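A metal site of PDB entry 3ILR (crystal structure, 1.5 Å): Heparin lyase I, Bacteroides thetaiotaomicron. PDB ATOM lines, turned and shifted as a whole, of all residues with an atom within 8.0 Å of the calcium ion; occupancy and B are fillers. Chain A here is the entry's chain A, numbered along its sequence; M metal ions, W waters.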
ATOM      1  N   GLN A 117      13.073 -28.945 -18.737  1.00  0.00           N
ATOM      2  CA  GLN A 117      12.715 -29.288 -17.374  1.00  0.00           C
ATOM      3  C   GLN A 117      13.674 -30.293 -16.796  1.00  0.00           C
ATOM      4  O   GLN A 117      14.049 -31.251 -17.477  1.00  0.00           O
ATOM      5  CB  GLN A 117      11.309 -29.912 -17.360  1.00  0.00           C
ATOM      6  CG  GLN A 117      10.174 -28.878 -17.387  1.00  0.00           C
ATOM      7  CD  GLN A 117      10.090 -28.109 -16.091  1.00  0.00           C
ATOM      8  OE1 GLN A 117       9.795 -26.906 -16.080  1.00  0.00           O
ATOM      9  NE2 GLN A 117      10.298 -28.797 -14.982  1.00  0.00           N
ATOM     10  N   MET A 147       8.780 -20.662 -18.880  1.00  0.00           N
ATOM     11  CA  MET A 147       8.163 -20.571 -20.213  1.00  0.00           C
ATOM     12  C   MET A 147       6.820 -21.313 -20.206  1.00  0.00           C
ATOM     13  O   MET A 147       6.578 -22.244 -20.977  1.00  0.00           O
ATOM     14  CB  MET A 147       9.126 -21.134 -21.286  1.00  0.00           C
ATOM     15  CG  MET A 147      10.492 -20.502 -21.277  1.00  0.00           C
ATOM     16  SD  MET A 147      11.555 -21.196 -22.555  1.00  0.00           S
ATOM     17  CE  MET A 147      10.707 -20.712 -24.076  1.00  0.00           C
ATOM     18  N   PRO A 148       5.895 -20.865 -19.351  1.00  0.00           N
ATOM     19  CA  PRO A 148       4.614 -21.569 -19.349  1.00  0.00           C
ATOM     20  C   PRO A 148       3.888 -21.411 -20.688  1.00  0.00           C
ATOM     21  O   PRO A 148       4.027 -20.399 -21.374  1.00  0.00           O
ATOM     22  CB  PRO A 148       3.826 -20.867 -18.220  1.00  0.00           C
ATOM     23  CG  PRO A 148       4.501 -19.531 -18.034  1.00  0.00           C
ATOM     24  CD  PRO A 148       5.977 -19.787 -18.354  1.00  0.00           C
ATOM     25  N   ASP A 149       3.086 -22.433 -20.996  1.00  0.00           N
ATOM     26  CA  ASP A 149       2.296 -22.503 -22.224  1.00  0.00           C
ATOM     27  C   ASP A 149       0.862 -22.268 -21.795  1.00  0.00           C
ATOM     28  O   ASP A 149       0.293 -23.057 -21.023  1.00  0.00           O
ATOM     29  CB  ASP A 149       2.489 -23.905 -22.814  1.00  0.00           C
ATOM     30  CG  ASP A 149       1.704 -24.143 -24.076  1.00  0.00           C
ATOM     31  OD1 ASP A 149       0.684 -23.433 -24.292  1.00  0.00           O
ATOM     32  OD2 ASP A 149       2.074 -25.058 -24.826  1.00  0.00           O
ATOM     33  N   LEU A 152      -2.397 -24.488 -21.261  1.00  0.00           N
ATOM     34  CA  LEU A 152      -2.819 -25.197 -20.044  1.00  0.00           C
ATOM     35  C   LEU A 152      -3.749 -24.229 -19.331  1.00  0.00           C
ATOM     36  O   LEU A 152      -3.364 -23.082 -18.973  1.00  0.00           O
ATOM     37  CB  LEU A 152      -1.657 -25.562 -19.157  1.00  0.00           C
ATOM     38  CG  LEU A 152      -2.106 -26.329 -17.909  1.00  0.00           C
ATOM     39  CD1 LEU A 152      -2.634 -27.715 -18.275  1.00  0.00           C
ATOM     40  CD2 LEU A 152      -0.960 -26.453 -16.934  1.00  0.00           C
ATOM     41  N   VAL A 160      -8.622 -28.355 -14.665  1.00  0.00           N
ATOM     42  CA  VAL A 160      -7.357 -27.975 -15.270  1.00  0.00           C
ATOM     43  C   VAL A 160      -7.098 -28.940 -16.446  1.00  0.00           C
ATOM     44  O   VAL A 160      -7.056 -30.157 -16.273  1.00  0.00           O
ATOM     45  CB  VAL A 160      -6.185 -28.048 -14.254  1.00  0.00           C
ATOM     46  CG1 VAL A 160      -4.839 -27.762 -14.913  1.00  0.00           C
ATOM     47  CG2 VAL A 160      -6.404 -27.091 -13.103  1.00  0.00           C
ATOM     48  N   GLU A 216      -2.349 -20.451 -18.089  1.00  0.00           N
ATOM     49  CA  GLU A 216      -1.067 -20.366 -17.386  1.00  0.00           C
ATOM     50  C   GLU A 216      -0.169 -19.330 -18.020  1.00  0.00           C
ATOM     51  O   GLU A 216       0.328 -19.515 -19.113  1.00  0.00           O
ATOM     52  CB  GLU A 216      -0.322 -21.693 -17.276  1.00  0.00           C
ATOM     53  CG  GLU A 216       0.718 -21.619 -16.141  1.00  0.00           C
ATOM     54  CD  GLU A 216       1.276 -22.984 -15.715  1.00  0.00           C
ATOM     55  OE1 GLU A 216       1.471 -23.870 -16.558  1.00  0.00           O
ATOM     56  OE2 GLU A 216       1.512 -23.194 -14.488  1.00  0.00           O
ATOM     57  N   GLN A 217       0.003 -18.225 -17.289  1.00  0.00           N
ATOM     58  CA  GLN A 217       0.726 -17.075 -17.784  1.00  0.00           C
ATOM     59  C   GLN A 217       1.480 -16.454 -16.630  1.00  0.00           C
ATOM     60  O   GLN A 217       1.008 -16.467 -15.498  1.00  0.00           O
ATOM     61  CB  GLN A 217      -0.263 -16.052 -18.316  1.00  0.00           C
ATOM     62  CG  GLN A 217       0.387 -14.771 -18.856  1.00  0.00           C
ATOM     63  CD  GLN A 217       0.712 -13.746 -17.794  1.00  0.00           C
ATOM     64  OE1 GLN A 217       1.671 -12.959 -17.966  1.00  0.00           O
ATOM     65  NE2 GLN A 217      -0.040 -13.748 -16.707  1.00  0.00           N
ATOM     66  N   ASP A 239       7.754 -23.593  -7.840  1.00  0.00           N
ATOM     67  CA  ASP A 239       6.273 -23.695  -7.858  1.00  0.00           C
ATOM     68  C   ASP A 239       5.944 -25.102  -8.298  1.00  0.00           C
ATOM     69  O   ASP A 239       6.138 -25.429  -9.463  1.00  0.00           O
ATOM     70  CB  ASP A 239       5.693 -22.680  -8.830  1.00  0.00           C
ATOM     71  CG  ASP A 239       4.162 -22.567  -8.748  1.00  0.00           C
ATOM     72  OD1 ASP A 239       3.522 -23.429  -8.130  1.00  0.00           O
ATOM     73  OD2 ASP A 239       3.628 -21.573  -9.324  1.00  0.00           O
ATOM     74  N   ARG A 240       5.414 -25.914  -7.398  1.00  0.00           N
ATOM     75  CA  ARG A 240       5.154 -27.321  -7.742  1.00  0.00           C
ATOM     76  C   ARG A 240       3.735 -27.527  -8.206  1.00  0.00           C
ATOM     77  O   ARG A 240       3.391 -28.634  -8.644  1.00  0.00           O
ATOM     78  CB  ARG A 240       5.457 -28.277  -6.584  1.00  0.00           C
ATOM     79  CG  ARG A 240       4.424 -28.266  -5.490  1.00  0.00           C
ATOM     80  CD  ARG A 240       4.776 -29.247  -4.336  1.00  0.00           C
ATOM     81  NE  ARG A 240       3.818 -29.032  -3.271  1.00  0.00           N
ATOM     82  CZ  ARG A 240       2.634 -29.622  -3.189  1.00  0.00           C
ATOM     83  NH1 ARG A 240       2.259 -30.494  -4.105  1.00  0.00           N
ATOM     84  NH2 ARG A 240       1.826 -29.326  -2.190  1.00  0.00           N
ATOM     85  N   LYS A 241       2.905 -26.507  -8.174  1.00  0.00           N
ATOM     86  CA  LYS A 241       1.526 -26.665  -8.637  1.00  0.00           C
ATOM     87  C   LYS A 241       1.525 -26.844 -10.146  1.00  0.00           C
ATOM     88  O   LYS A 241       2.361 -26.281 -10.842  1.00  0.00           O
ATOM     89  CB  LYS A 241       0.662 -25.473  -8.229  1.00  0.00           C
ATOM     90  CG  LYS A 241      -0.828 -25.801  -8.196  1.00  0.00           C
ATOM     91  CD  LYS A 241      -1.659 -24.620  -7.629  1.00  0.00           C
ATOM     92  CE  LYS A 241      -2.962 -25.137  -7.042  1.00  0.00           C
ATOM     93  NZ  LYS A 241      -3.914 -24.031  -6.782  1.00  0.00           N
ATOM     94  N   TRP A 242       0.641 -27.690 -10.660  1.00  0.00           N
ATOM     95  CA  TRP A 242       0.643 -27.925 -12.101  1.00  0.00           C
ATOM     96  C   TRP A 242       0.174 -26.683 -12.858  1.00  0.00           C
ATOM     97  O   TRP A 242       0.862 -26.264 -13.791  1.00  0.00           O
ATOM     98  CB  TRP A 242      -0.187 -29.180 -12.414  1.00  0.00           C
ATOM     99  CG  TRP A 242      -0.293 -29.543 -13.847  1.00  0.00           C
ATOM    100  CD1 TRP A 242      -1.456 -29.775 -14.528  1.00  0.00           C
ATOM    101  CD2 TRP A 242       0.770 -29.830 -14.773  1.00  0.00           C
ATOM    102  NE1 TRP A 242      -1.181 -30.136 -15.834  1.00  0.00           N
ATOM    103  CE2 TRP A 242       0.172 -30.170 -16.006  1.00  0.00           C
ATOM    104  CE3 TRP A 242       2.147 -29.769 -14.687  1.00  0.00           C
ATOM    105  CZ2 TRP A 242       0.927 -30.493 -17.120  1.00  0.00           C
ATOM    106  CZ3 TRP A 242       2.898 -30.084 -15.812  1.00  0.00           C
ATOM    107  CH2 TRP A 242       2.284 -30.448 -17.009  1.00  0.00           C
ATOM    108  N   LEU A 243      -0.940 -26.102 -12.428  1.00  0.00           N
ATOM    109  CA  LEU A 243      -1.343 -24.779 -12.889  1.00  0.00           C
ATOM    110  C   LEU A 243      -1.025 -23.771 -11.800  1.00  0.00           C
ATOM    111  O   LEU A 243      -1.622 -23.776 -10.722  1.00  0.00           O
ATOM    112  CB  LEU A 243      -2.831 -24.720 -13.243  1.00  0.00           C
ATOM    113  CG  LEU A 243      -3.353 -23.333 -13.620  1.00  0.00           C
ATOM    114  CD1 LEU A 243      -2.688 -22.807 -14.906  1.00  0.00           C
ATOM    115  CD2 LEU A 243      -4.886 -23.313 -13.833  1.00  0.00           C
ATOM    116  N   THR A 244      -0.062 -22.911 -12.067  1.00  0.00           N
ATOM    117  CA  THR A 244       0.341 -21.929 -11.055  1.00  0.00           C
ATOM    118  C   THR A 244      -0.855 -21.102 -10.600  1.00  0.00           C
ATOM    119  O   THR A 244      -1.671 -20.649 -11.401  1.00  0.00           O
ATOM    120  CB  THR A 244       1.377 -20.997 -11.670  1.00  0.00           C
ATOM    121  OG1 THR A 244       2.627 -21.682 -11.733  1.00  0.00           O
ATOM    122  CG2 THR A 244       1.532 -19.729 -10.847  1.00  0.00           C
ATOM    123  N   ASP A 245      -0.921 -20.877  -9.285  1.00  0.00           N
ATOM    124  CA  ASP A 245      -1.917 -19.988  -8.673  1.00  0.00           C
ATOM    125  C   ASP A 245      -1.328 -18.591  -8.468  1.00  0.00           C
ATOM    126  O   ASP A 245      -0.504 -18.377  -7.570  1.00  0.00           O
ATOM    127  CB  ASP A 245      -2.330 -20.587  -7.342  1.00  0.00           C
ATOM    128  CG  ASP A 245      -3.410 -19.800  -6.643  1.00  0.00           C
ATOM    129  OD1 ASP A 245      -3.749 -18.714  -7.141  1.00  0.00           O
ATOM    130  OD2 ASP A 245      -3.884 -20.317  -5.594  1.00  0.00           O
ATOM    131  N   LYS A 300       4.695 -33.243 -12.658  1.00  0.00           N
ATOM    132  CA  LYS A 300       3.635 -32.836 -13.604  1.00  0.00           C
ATOM    133  C   LYS A 300       2.288 -32.843 -12.881  1.00  0.00           C
ATOM    134  O   LYS A 300       2.169 -32.241 -11.821  1.00  0.00           O
ATOM    135  CB  LYS A 300       3.623 -33.708 -14.866  1.00  0.00           C
ATOM    136  CG  LYS A 300       4.933 -33.592 -15.648  1.00  0.00           C
ATOM    137  CD  LYS A 300       4.780 -33.972 -17.103  1.00  0.00           C
ATOM    138  N   GLU A 303       2.152 -33.260  -9.137  1.00  0.00           N
ATOM    139  CA  GLU A 303       2.568 -32.112  -8.302  1.00  0.00           C
ATOM    140  C   GLU A 303       3.597 -32.470  -7.247  1.00  0.00           C
ATOM    141  O   GLU A 303       3.783 -31.739  -6.278  1.00  0.00           O
ATOM    142  CB  GLU A 303       1.351 -31.395  -7.718  1.00  0.00           C
ATOM    143  CG  GLU A 303       0.494 -30.791  -8.800  1.00  0.00           C
ATOM    144  CD  GLU A 303      -0.711 -30.032  -8.292  1.00  0.00           C
ATOM    145  OE1 GLU A 303      -1.227 -30.413  -7.220  1.00  0.00           O
ATOM    146  OE2 GLU A 303      -1.153 -29.072  -8.955  1.00  0.00           O
ATOM    147  N   ARG A 338       9.736 -24.438 -12.017  1.00  0.00           N
ATOM    148  CA  ARG A 338       8.278 -24.374 -12.150  1.00  0.00           C
ATOM    149  C   ARG A 338       7.825 -25.708 -12.659  1.00  0.00           C
ATOM    150  O   ARG A 338       8.481 -26.304 -13.540  1.00  0.00           O
ATOM    151  CB  ARG A 338       7.875 -23.377 -13.221  1.00  0.00           C
ATOM    152  CG  ARG A 338       8.087 -21.928 -12.832  1.00  0.00           C
ATOM    153  CD  ARG A 338       7.702 -20.960 -13.974  1.00  0.00           C
ATOM    154  NE  ARG A 338       6.432 -21.374 -14.528  1.00  0.00           N
ATOM    155  CZ  ARG A 338       5.253 -21.075 -14.002  1.00  0.00           C
ATOM    156  NH1 ARG A 338       5.161 -20.254 -12.939  1.00  0.00           N
ATOM    157  NH2 ARG A 338       4.145 -21.588 -14.543  1.00  0.00           N
ATOM    158  N   ASN A 339       6.717 -26.198 -12.134  1.00  0.00           N
ATOM    159  CA  ASN A 339       6.102 -27.396 -12.674  1.00  0.00           C
ATOM    160  C   ASN A 339       5.365 -27.128 -13.976  1.00  0.00           C
ATOM    161  O   ASN A 339       4.147 -26.903 -13.965  1.00  0.00           O
ATOM    162  CB  ASN A 339       5.165 -27.987 -11.622  1.00  0.00           C
ATOM    163  CG  ASN A 339       4.636 -29.362 -12.017  1.00  0.00           C
ATOM    164  OD1 ASN A 339       5.095 -29.975 -13.010  1.00  0.00           O
ATOM    165  ND2 ASN A 339       3.681 -29.870 -11.207  1.00  0.00           N
ATOM    166  N   ASP A 340       6.134 -27.098 -15.068  1.00  0.00           N
ATOM    167  CA  ASP A 340       5.609 -26.854 -16.432  1.00  0.00           C
ATOM    168  C   ASP A 340       6.108 -27.962 -17.346  1.00  0.00           C
ATOM    169  O   ASP A 340       7.035 -28.726 -17.010  1.00  0.00           O
ATOM    170  CB  ASP A 340       6.191 -25.566 -16.995  1.00  0.00           C
ATOM    171  CG  ASP A 340       5.623 -24.290 -16.357  1.00  0.00           C
ATOM    172  OD1 ASP A 340       4.590 -24.352 -15.678  1.00  0.00           O
ATOM    173  OD2 ASP A 340       6.209 -23.203 -16.548  1.00  0.00           O
ATOM    174  N   GLU A 341       5.486 -28.043 -18.510  1.00  0.00           N
ATOM    175  CA  GLU A 341       6.020 -28.898 -19.560  1.00  0.00           C
ATOM    176  C   GLU A 341       7.324 -28.336 -20.091  1.00  0.00           C
ATOM    177  O   GLU A 341       8.258 -29.109 -20.399  1.00  0.00           O
ATOM    178  CB  GLU A 341       5.004 -29.031 -20.695  1.00  0.00           C
ATOM    179  CG  GLU A 341       5.179 -30.331 -21.445  1.00  0.00           C
ATOM    180  CD  GLU A 341       4.698 -31.511 -20.606  1.00  0.00           C
ATOM    181  OE1 GLU A 341       3.473 -31.655 -20.393  1.00  0.00           O
ATOM    182  OE2 GLU A 341       5.553 -32.285 -20.122  1.00  0.00           O
ATOM    183  N   ASP A 342       7.402 -27.003 -20.230  1.00  0.00           N
ATOM    184  CA  ASP A 342       8.561 -26.349 -20.864  1.00  0.00           C
ATOM    185  C   ASP A 342       9.542 -25.824 -19.846  1.00  0.00           C
ATOM    186  O   ASP A 342       9.258 -25.830 -18.635  1.00  0.00           O
ATOM    187  CB  ASP A 342       8.046 -25.237 -21.785  1.00  0.00           C
ATOM    188  CG  ASP A 342       7.063 -25.766 -22.834  1.00  0.00           C
ATOM    189  OD1 ASP A 342       7.503 -26.578 -23.673  1.00  0.00           O
ATOM    190  OD2 ASP A 342       5.888 -25.389 -22.822  1.00  0.00           O
HETATM  191 CA    CA M   1       2.650 -25.241 -14.739  1.00  0.00          CA
HETATM  192  O   HOH W   1       3.317 -24.346 -12.546  1.00  0.00           O
HETATM  193  O   HOH W   2       2.263 -26.902 -16.388  1.00  0.00           O
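The side-chain carboxylate (OE2) of Glu 303 lies within hydrogen-bond range of the backbone NH (N) of Trp 242. The side-chain carboxylate of Asp 340 lies within salt-bridge range of the guanidinium group of Arg 338 (2.7 Å). The backbone carbonyl oxygen (O) of Asp 340 lies close to the side-chain amide oxygen (OE1) of Gln 117 (3.4 Å). The guanidinium group (NH2) of Arg 338 lies close to the side-chain carboxylate (OE2) of Glu 216. The backbone carbonyl oxygen (O) of Leu 152 lies within hydrogen-bond range of the backbone NH (N) of Glu 216, at 3.0 Å. The backbone NH (N) of Asn 339 sits at hydrogen-bond distance from the backbone carbonyl oxygen (O) of Asp 239, at 2.8 Å. The guanidinium group of Arg 338 sits at hydrogen-bond distance from the side-chain hydroxyl of Thr 244. The backbone carbonyl oxygen of Arg 338 sits close to the side-chain amide oxygen of Gln 117.
Arg 338 touches the calcium ion (NH2 to CA, 3.95 Å). Five residues have an atom within 4 Å of the calcium ion: Glu 216, Trp 242, Arg 338, Asn 339 and Asp 340. The nearest printed residue that does not touch the calcium ion is Lys 241 (4.04 Å).
The calcium ion is bound by the backbone carbonyl oxygen (O) of Trp 242 (2.3 Å), the side-chain carboxylate (OD1) of Asp 340 (2.3 Å), the side-chain carboxylate (OE2) of Glu 216 (2.4 Å), the backbone carbonyl oxygen (O) of Asn 339 (2.4 Å), water W2 (2.4 Å), water W1 (2.5 Å) and the side-chain carboxylate (OE1) of Glu 216 (2.6 Å).
Water W1 bridges the backbone carbonyl oxygen of Lys 241 (2.7 Å) and the side-chain hydroxyl of Thr 244 (2.9 Å).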
